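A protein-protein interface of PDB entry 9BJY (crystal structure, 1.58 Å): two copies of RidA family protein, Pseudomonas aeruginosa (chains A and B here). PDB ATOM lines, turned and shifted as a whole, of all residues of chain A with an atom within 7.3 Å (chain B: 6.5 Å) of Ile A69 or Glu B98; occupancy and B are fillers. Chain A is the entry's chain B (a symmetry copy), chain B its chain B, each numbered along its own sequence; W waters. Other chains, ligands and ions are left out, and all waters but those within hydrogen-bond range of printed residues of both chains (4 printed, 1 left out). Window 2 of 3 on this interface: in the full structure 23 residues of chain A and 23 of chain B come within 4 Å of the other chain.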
ATOM      1  N   ILE A  64      10.830  20.519  15.677  1.00  0.00           N
ATOM      2  CA  ILE A  64      10.690  20.594  14.236  1.00  0.00           C
ATOM      3  C   ILE A  64      11.541  19.483  13.652  1.00  0.00           C
ATOM      4  O   ILE A  64      12.767  19.474  13.828  1.00  0.00           O
ATOM      5  CB  ILE A  64      11.128  21.957  13.693  1.00  0.00           C
ATOM      6  CG1 ILE A  64      10.256  23.062  14.320  1.00  0.00           C
ATOM      7  CG2 ILE A  64      11.045  21.976  12.177  1.00  0.00           C
ATOM      8  CD1 ILE A  64      10.685  24.474  13.970  1.00  0.00           C
ATOM      9  N   TYR A  65      10.891  18.572  12.960  1.00  0.00           N
ATOM     10  CA  TYR A  65      11.538  17.450  12.294  1.00  0.00           C
ATOM     11  C   TYR A  65      11.614  17.770  10.811  1.00  0.00           C
ATOM     12  O   TYR A  65      10.588  18.066  10.189  1.00  0.00           O
ATOM     13  CB  TYR A  65      10.781  16.146  12.498  1.00  0.00           C
ATOM     14  CG  TYR A  65      10.627  15.723  13.934  1.00  0.00           C
ATOM     15  CD1 TYR A  65      11.646  15.053  14.587  1.00  0.00           C
ATOM     16  CD2 TYR A  65       9.453  15.971  14.626  1.00  0.00           C
ATOM     17  CE1 TYR A  65      11.507  14.659  15.899  1.00  0.00           C
ATOM     18  CE2 TYR A  65       9.306  15.575  15.944  1.00  0.00           C
ATOM     19  CZ  TYR A  65      10.346  14.908  16.564  1.00  0.00           C
ATOM     20  OH  TYR A  65      10.234  14.476  17.865  1.00  0.00           O
ATOM     21  N   LEU A  66      12.808  17.713  10.261  1.00  0.00           N
ATOM     22  CA  LEU A  66      13.007  17.864   8.826  1.00  0.00           C
ATOM     23  C   LEU A  66      13.535  16.568   8.240  1.00  0.00           C
ATOM     24  O   LEU A  66      14.488  15.994   8.761  1.00  0.00           O
ATOM     25  CB  LEU A  66      13.972  19.004   8.507  1.00  0.00           C
ATOM     26  CG  LEU A  66      13.433  20.399   8.796  1.00  0.00           C
ATOM     27  CD1 LEU A  66      14.510  21.442   8.686  1.00  0.00           C
ATOM     28  CD2 LEU A  66      12.303  20.685   7.864  1.00  0.00           C
ATOM     29  N   LYS A  67      12.936  16.127   7.138  1.00  0.00           N
ATOM     30  CA  LYS A  67      13.457  14.959   6.447  1.00  0.00           C
ATOM     31  C   LYS A  67      14.912  15.152   6.028  1.00  0.00           C
ATOM     32  O   LYS A  67      15.717  14.214   6.097  1.00  0.00           O
ATOM     33  CB  LYS A  67      12.598  14.662   5.222  1.00  0.00           C
ATOM     34  CG  LYS A  67      12.917  13.336   4.607  1.00  0.00           C
ATOM     35  CD  LYS A  67      12.327  13.165   3.249  1.00  0.00           C
ATOM     36  CE  LYS A  67      12.579  11.726   2.837  1.00  0.00           C
ATOM     37  NZ  LYS A  67      13.033  11.625   1.454  1.00  0.00           N
ATOM     38  N   ASP A  68      15.269  16.360   5.579  1.00  0.00           N
ATOM     39  CA  ASP A  68      16.633  16.689   5.148  1.00  0.00           C
ATOM     40  C   ASP A  68      16.986  18.050   5.732  1.00  0.00           C
ATOM     41  O   ASP A  68      16.597  19.089   5.175  1.00  0.00           O
ATOM     42  CB  ASP A  68      16.741  16.679   3.630  1.00  0.00           C
ATOM     43  CG  ASP A  68      18.157  16.797   3.150  1.00  0.00           C
ATOM     44  OD1 ASP A  68      18.980  17.427   3.832  1.00  0.00           O
ATOM     45  OD2 ASP A  68      18.467  16.241   2.083  1.00  0.00           O
ATOM     46  N   ILE A  69      17.663  18.048   6.887  1.00  0.00           N
ATOM     47  CA  ILE A  69      17.900  19.302   7.589  1.00  0.00           C
ATOM     48  C   ILE A  69      18.902  20.175   6.837  1.00  0.00           C
ATOM     49  O   ILE A  69      18.773  21.397   6.831  1.00  0.00           O
ATOM     50  CB  ILE A  69      18.319  19.019   9.045  1.00  0.00           C
ATOM     51  CG1 ILE A  69      18.206  20.287   9.889  1.00  0.00           C
ATOM     52  CG2 ILE A  69      19.717  18.392   9.116  1.00  0.00           C
ATOM     53  CD1 ILE A  69      18.242  20.007  11.387  1.00  0.00           C
ATOM     54  N   ALA A  70      19.894  19.586   6.167  1.00  0.00           N
ATOM     55  CA  ALA A  70      20.832  20.425   5.426  1.00  0.00           C
ATOM     56  C   ALA A  70      20.135  21.124   4.264  1.00  0.00           C
ATOM     57  O   ALA A  70      20.389  22.299   3.985  1.00  0.00           O
ATOM     58  CB  ALA A  70      21.999  19.579   4.918  1.00  0.00           C
ATOM     59  N   ARG A  71      19.250  20.419   3.577  1.00  0.00           N
ATOM     60  CA  ARG A  71      18.637  20.963   2.373  1.00  0.00           C
ATOM     61  C   ARG A  71      17.574  22.002   2.685  1.00  0.00           C
ATOM     62  O   ARG A  71      17.449  23.006   1.963  1.00  0.00           O
ATOM     63  CB  ARG A  71      18.033  19.816   1.570  1.00  0.00           C
ATOM     64  CG  ARG A  71      17.477  20.140   0.205  1.00  0.00           C
ATOM     65  CD  ARG A  71      17.216  18.822  -0.518  1.00  0.00           C
ATOM     66  NE  ARG A  71      16.709  18.957  -1.875  1.00  0.00           N
ATOM     67  CZ  ARG A  71      16.555  17.930  -2.706  1.00  0.00           C
ATOM     68  NH1 ARG A  71      16.853  16.690  -2.335  1.00  0.00           N
ATOM     69  NH2 ARG A  71      16.105  18.154  -3.936  1.00  0.00           N
ATOM     70  N   ASP A  72      16.811  21.779   3.753  1.00  0.00           N
ATOM     71  CA  ASP A  72      15.537  22.464   3.945  1.00  0.00           C
ATOM     72  C   ASP A  72      15.459  23.379   5.162  1.00  0.00           C
ATOM     73  O   ASP A  72      14.446  24.066   5.329  1.00  0.00           O
ATOM     74  CB  ASP A  72      14.413  21.425   4.059  1.00  0.00           C
ATOM     75  CG  ASP A  72      14.115  20.728   2.755  1.00  0.00           C
ATOM     76  OD1 ASP A  72      14.317  21.321   1.674  1.00  0.00           O
ATOM     77  OD2 ASP A  72      13.638  19.577   2.803  1.00  0.00           O
ATOM     78  N   PHE A  73      16.512  23.458   5.977  1.00  0.00           N
ATOM     79  CA  PHE A  73      16.484  24.289   7.171  1.00  0.00           C
ATOM     80  C   PHE A  73      16.264  25.754   6.827  1.00  0.00           C
ATOM     81  O   PHE A  73      15.524  26.455   7.532  1.00  0.00           O
ATOM     82  CB  PHE A  73      17.800  24.118   7.932  1.00  0.00           C
ATOM     83  CG  PHE A  73      17.802  24.702   9.308  1.00  0.00           C
ATOM     84  CD1 PHE A  73      16.766  24.461  10.185  1.00  0.00           C
ATOM     85  CD2 PHE A  73      18.895  25.417   9.758  1.00  0.00           C
ATOM     86  CE1 PHE A  73      16.788  24.967  11.469  1.00  0.00           C
ATOM     87  CE2 PHE A  73      18.937  25.910  11.047  1.00  0.00           C
ATOM     88  CZ  PHE A  73      17.887  25.674  11.907  1.00  0.00           C
ATOM     89  N   ALA A  74      16.927  26.254   5.779  1.00  0.00           N
ATOM     90  CA  ALA A  74      16.812  27.673   5.461  1.00  0.00           C
ATOM     91  C   ALA A  74      15.383  28.031   5.095  1.00  0.00           C
ATOM     92  O   ALA A  74      14.852  29.049   5.567  1.00  0.00           O
ATOM     93  CB  ALA A  74      17.761  28.057   4.316  1.00  0.00           C
ATOM     94  N   THR A  93      13.499  23.068  18.969  1.00  0.00           N
ATOM     95  CA  THR A  93      14.566  22.133  18.631  1.00  0.00           C
ATOM     96  C   THR A  93      14.291  21.692  17.202  1.00  0.00           C
ATOM     97  O   THR A  93      13.174  21.282  16.897  1.00  0.00           O
ATOM     98  CB  THR A  93      14.527  20.919  19.564  1.00  0.00           C
ATOM     99  OG1 THR A  93      14.685  21.357  20.910  1.00  0.00           O
ATOM    100  CG2 THR A  93      15.606  19.916  19.218  1.00  0.00           C
ATOM    101  N   THR A  94      15.293  21.756  16.328  1.00  0.00           N
ATOM    102  CA  THR A  94      15.140  21.322  14.946  1.00  0.00           C
ATOM    103  C   THR A  94      16.142  20.211  14.654  1.00  0.00           C
ATOM    104  O   THR A  94      17.353  20.401  14.830  1.00  0.00           O
ATOM    105  CB  THR A  94      15.339  22.485  13.977  1.00  0.00           C
ATOM    106  OG1 THR A  94      14.524  23.582  14.397  1.00  0.00           O
ATOM    107  CG2 THR A  94      14.922  22.061  12.576  1.00  0.00           C
ATOM    108  N   VAL A  95      15.639  19.046  14.248  1.00  0.00           N
ATOM    109  CA  VAL A  95      16.481  17.886  13.982  1.00  0.00           C
ATOM    110  C   VAL A  95      15.990  17.178  12.724  1.00  0.00           C
ATOM    111  O   VAL A  95      14.861  17.366  12.263  1.00  0.00           O
ATOM    112  CB  VAL A  95      16.515  16.904  15.175  1.00  0.00           C
ATOM    113  CG1 VAL A  95      16.843  17.637  16.475  1.00  0.00           C
ATOM    114  CG2 VAL A  95      15.172  16.167  15.300  1.00  0.00           C
ATOM    115  N   GLN A  96      16.859  16.325  12.183  1.00  0.00           N
ATOM    116  CA  GLN A  96      16.518  15.509  11.042  1.00  0.00           C
ATOM    117  C   GLN A  96      15.929  14.172  11.471  1.00  0.00           C
ATOM    118  O   GLN A  96      16.452  13.489  12.362  1.00  0.00           O
ATOM    119  CB  GLN A  96      17.760  15.261  10.194  1.00  0.00           C
ATOM    120  CG  GLN A  96      17.507  14.437   8.997  1.00  0.00           C
ATOM    121  CD  GLN A  96      18.642  14.483   8.020  1.00  0.00           C
ATOM    122  OE1 GLN A  96      18.878  15.492   7.359  1.00  0.00           O
ATOM    123  NE2 GLN A  96      19.374  13.384   7.926  1.00  0.00           N
ATOM    124  N   ALA A  97      14.861  13.788  10.791  1.00  0.00           N
ATOM    125  CA  ALA A  97      14.215  12.507  10.956  1.00  0.00           C
ATOM    126  C   ALA A  97      13.314  12.265   9.765  1.00  0.00           C
ATOM    127  O   ALA A  97      12.598  13.177   9.339  1.00  0.00           O
ATOM    128  CB  ALA A  97      13.374  12.458  12.242  1.00  0.00           C
ATOM    129  N   LEU A 105       8.231  16.393   4.183  1.00  0.00           N
ATOM    130  CA  LEU A 105       9.531  17.003   4.404  1.00  0.00           C
ATOM    131  C   LEU A 105       9.668  17.628   5.784  1.00  0.00           C
ATOM    132  O   LEU A 105      10.794  17.880   6.219  1.00  0.00           O
ATOM    133  CB  LEU A 105       9.809  18.090   3.355  1.00  0.00           C
ATOM    134  CG  LEU A 105       9.654  17.550   1.934  1.00  0.00           C
ATOM    135  CD1 LEU A 105       9.829  18.686   0.922  1.00  0.00           C
ATOM    136  CD2 LEU A 105      10.584  16.392   1.624  1.00  0.00           C
ATOM    137  N   LEU B  66      22.145  12.563  19.237  1.00  0.00           N
ATOM    138  CA  LEU B  66      23.513  12.341  18.787  1.00  0.00           C
ATOM    139  C   LEU B  66      23.541  12.194  17.277  1.00  0.00           C
ATOM    140  O   LEU B  66      22.760  11.432  16.713  1.00  0.00           O
ATOM    141  CB  LEU B  66      24.126  11.101  19.436  1.00  0.00           C
ATOM    142  CG  LEU B  66      24.409  11.233  20.927  1.00  0.00           C
ATOM    143  CD1 LEU B  66      24.782   9.909  21.537  1.00  0.00           C
ATOM    144  CD2 LEU B  66      25.485  12.247  21.128  1.00  0.00           C
ATOM    145  N   LYS B  67      24.463  12.900  16.630  1.00  0.00           N
ATOM    146  CA  LYS B  67      24.636  12.727  15.197  1.00  0.00           C
ATOM    147  C   LYS B  67      24.956  11.279  14.837  1.00  0.00           C
ATOM    148  O   LYS B  67      24.478  10.763  13.818  1.00  0.00           O
ATOM    149  CB  LYS B  67      25.749  13.643  14.700  1.00  0.00           C
ATOM    150  CG  LYS B  67      25.814  13.708  13.207  1.00  0.00           C
ATOM    151  CD  LYS B  67      27.069  14.332  12.702  1.00  0.00           C
ATOM    152  CE  LYS B  67      26.912  14.490  11.201  1.00  0.00           C
ATOM    153  NZ  LYS B  67      28.116  14.091  10.480  1.00  0.00           N
ATOM    154  N   GLN B  96      19.475   9.036  17.664  1.00  0.00           N
ATOM    155  CA  GLN B  96      20.274   9.597  16.601  1.00  0.00           C
ATOM    156  C   GLN B  96      19.453  10.529  15.721  1.00  0.00           C
ATOM    157  O   GLN B  96      18.331  10.207  15.307  1.00  0.00           O
ATOM    158  CB  GLN B  96      20.854   8.478  15.744  1.00  0.00           C
ATOM    159  CG  GLN B  96      21.695   8.959  14.631  1.00  0.00           C
ATOM    160  CD  GLN B  96      22.509   7.862  14.014  1.00  0.00           C
ATOM    161  OE1 GLN B  96      23.463   7.362  14.608  1.00  0.00           O
ATOM    162  NE2 GLN B  96      22.132   7.462  12.810  1.00  0.00           N
ATOM    163  N   ALA B  97      20.049  11.667  15.402  1.00  0.00           N
ATOM    164  CA  ALA B  97      19.497  12.641  14.488  1.00  0.00           C
ATOM    165  C   ALA B  97      20.603  13.582  14.063  1.00  0.00           C
ATOM    166  O   ALA B  97      21.393  14.021  14.903  1.00  0.00           O
ATOM    167  CB  ALA B  97      18.366  13.452  15.139  1.00  0.00           C
ATOM    168  N   GLU B  98      20.644  13.897  12.772  1.00  0.00           N
ATOM    169  CA  GLU B  98      21.506  14.976  12.304  1.00  0.00           C
ATOM    170  C   GLU B  98      20.978  16.317  12.808  1.00  0.00           C
ATOM    171  O   GLU B  98      19.768  16.560  12.840  1.00  0.00           O
ATOM    172  CB  GLU B  98      21.593  14.986  10.775  1.00  0.00           C
ATOM    173  CG  GLU B  98      22.548  16.049  10.231  1.00  0.00           C
ATOM    174  CD  GLU B  98      23.298  15.602   8.988  1.00  0.00           C
ATOM    175  OE1 GLU B  98      23.687  14.421   8.929  1.00  0.00           O
ATOM    176  OE2 GLU B  98      23.485  16.436   8.079  1.00  0.00           O
ATOM    177  N   LEU B  99      21.891  17.183  13.224  1.00  0.00           N
ATOM    178  CA  LEU B  99      21.546  18.493  13.736  1.00  0.00           C
ATOM    179  C   LEU B  99      21.711  19.536  12.628  1.00  0.00           C
ATOM    180  O   LEU B  99      22.094  19.235  11.495  1.00  0.00           O
ATOM    181  CB  LEU B  99      22.370  18.794  14.982  1.00  0.00           C
ATOM    182  CG  LEU B  99      22.152  17.932  16.229  1.00  0.00           C
ATOM    183  CD1 LEU B  99      20.674  17.606  16.469  1.00  0.00           C
ATOM    184  CD2 LEU B  99      22.963  16.647  16.182  1.00  0.00           C
ATOM    185  N   ALA B 100      21.382  20.778  12.954  1.00  0.00           N
ATOM    186  CA  ALA B 100      21.214  21.773  11.894  1.00  0.00           C
ATOM    187  C   ALA B 100      22.539  22.143  11.242  1.00  0.00           C
ATOM    188  O   ALA B 100      22.560  22.516  10.060  1.00  0.00           O
ATOM    189  CB  ALA B 100      20.535  23.017  12.446  1.00  0.00           C
ATOM    190  N   ARG B 101      23.648  22.032  11.977  1.00  0.00           N
ATOM    191  CA  ARG B 101      24.959  22.266  11.375  1.00  0.00           C
ATOM    192  C   ARG B 101      25.772  20.975  11.427  1.00  0.00           C
ATOM    193  O   ARG B 101      25.731  20.259  12.436  1.00  0.00           O
ATOM    194  CB  ARG B 101      25.706  23.390  12.111  1.00  0.00           C
ATOM    195  CG  ARG B 101      25.142  24.794  11.868  1.00  0.00           C
ATOM    196  CD  ARG B 101      24.050  25.150  12.890  1.00  0.00           C
ATOM    197  NE  ARG B 101      23.484  26.474  12.653  1.00  0.00           N
ATOM    198  CZ  ARG B 101      22.410  26.958  13.267  1.00  0.00           C
ATOM    199  NH1 ARG B 101      21.770  26.267  14.193  1.00  0.00           N
ATOM    200  NH2 ARG B 101      21.973  28.173  12.945  1.00  0.00           N
ATOM    201  N   PRO B 102      26.519  20.649  10.364  1.00  0.00           N
ATOM    202  CA  PRO B 102      27.158  19.325  10.295  1.00  0.00           C
ATOM    203  C   PRO B 102      28.233  19.084  11.337  1.00  0.00           C
ATOM    204  O   PRO B 102      28.507  17.912  11.644  1.00  0.00           O
ATOM    205  CB  PRO B 102      27.748  19.288   8.872  1.00  0.00           C
ATOM    206  CG  PRO B 102      26.984  20.340   8.112  1.00  0.00           C
ATOM    207  CD  PRO B 102      26.682  21.412   9.112  1.00  0.00           C
ATOM    208  N   VAL B 104      27.963  19.697  14.469  1.00  0.00           N
ATOM    209  CA  VAL B 104      27.352  19.435  15.764  1.00  0.00           C
ATOM    210  C   VAL B 104      27.157  17.937  15.930  1.00  0.00           C
ATOM    211  O   VAL B 104      26.449  17.301  15.140  1.00  0.00           O
ATOM    212  CB  VAL B 104      26.009  20.177  15.884  1.00  0.00           C
ATOM    213  CG1 VAL B 104      25.314  19.795  17.142  1.00  0.00           C
ATOM    214  CG2 VAL B 104      26.220  21.697  15.797  1.00  0.00           C
HETATM  215  O   HOH W   1      19.849  21.348  15.331  1.00  0.00           O
HETATM  216  O   HOH W   2      16.721  10.710  12.993  1.00  0.00           O
HETATM  217  O   HOH W   3      21.197  23.108   7.991  1.00  0.00           O
HETATM  218  O   HOH W   4      21.923  13.494   6.529  1.00  0.00           O
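N of Gln A96 lies within hydrogen-bond range of O of Glu B98.
N of Ala B97 lies within hydrogen-bond range of O of Leu B66, 3.0 Å away. The backbone NH (N) of Val A95 sits at hydrogen-bond distance from the backbone carbonyl oxygen (O) of Ile A64, at 2.9 Å. N of Leu A66 sits at hydrogen-bond distance from O of Val A95 (2.9 Å). The backbone NH (N) of Ile A69 lies within hydrogen-bond range of the side-chain amide oxygen (OE1) of Gln A96 (2.9 Å).
Among the printed residues, pairs that only touch across the chains: Ile A69 with Glu B98, Ile A69 with Leu B99, Ile A69 with Ala B100, Phe A73 with Ala B100, Val A95 with Ala B97, Val A95 with Glu B98, Val A95 with Leu B99 and Gln A96 with Ala B97.
Asp A68 touches none of the printed residues of chain B. Ile A69 touches three residues of chain B. Asp A72 touches none of the printed residues of chain B. Of the printed residues of chain B, Phe A73 touches Ala B100 (3.6 Å). Of the printed residues of chain A, Ala B97 touches Val A95 (3.9 Å) and Gln A96 (3.4 Å). Printed residues of chain A within 4 Å of Glu B98: Ile A69 (3.8 Å), Val A95 (3.7 Å) and Gln A96 (3.0 Å). Of the printed residues of chain A, Leu B99 touches Ile A69 (3.5 Å) and Val A95 (3.8 Å). Printed residues of chain A within 4 Å of Ala B100: Ile A69 and Phe A73. The nearest residue of chain B that does not touch Ile A69 is Arg B101 (5.8 Å).
Of the 17 printed residues of chain A, 4 touch a printed residue of chain B. Along chain A the printed residues that touch a printed residue of chain B span positions 69 to 96.
Gln A96 touches Ala B97, but with the chains exchanged Ala A97 does not touch Gln B96 (6.2 Å). Of the 9 pairs that touch across the chains among the printed residues, none has its exchanged pair printed and touching as well.
Water W3 lies within hydrogen-bond range of O of Ala B100 and O of Ile A69. Water W1 bridges the backbone carbonyl oxygen of Thr A94 (2.7 Å) and the backbone NH of Ala B100 (2.9 Å). Water W2 lies within hydrogen-bond range of O of Gln A96 and O of Gln B96. Water W4 bridges NE2 of Gln A96 (2.9 Å) and OE1 of Glu B98 (3.1 Å).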
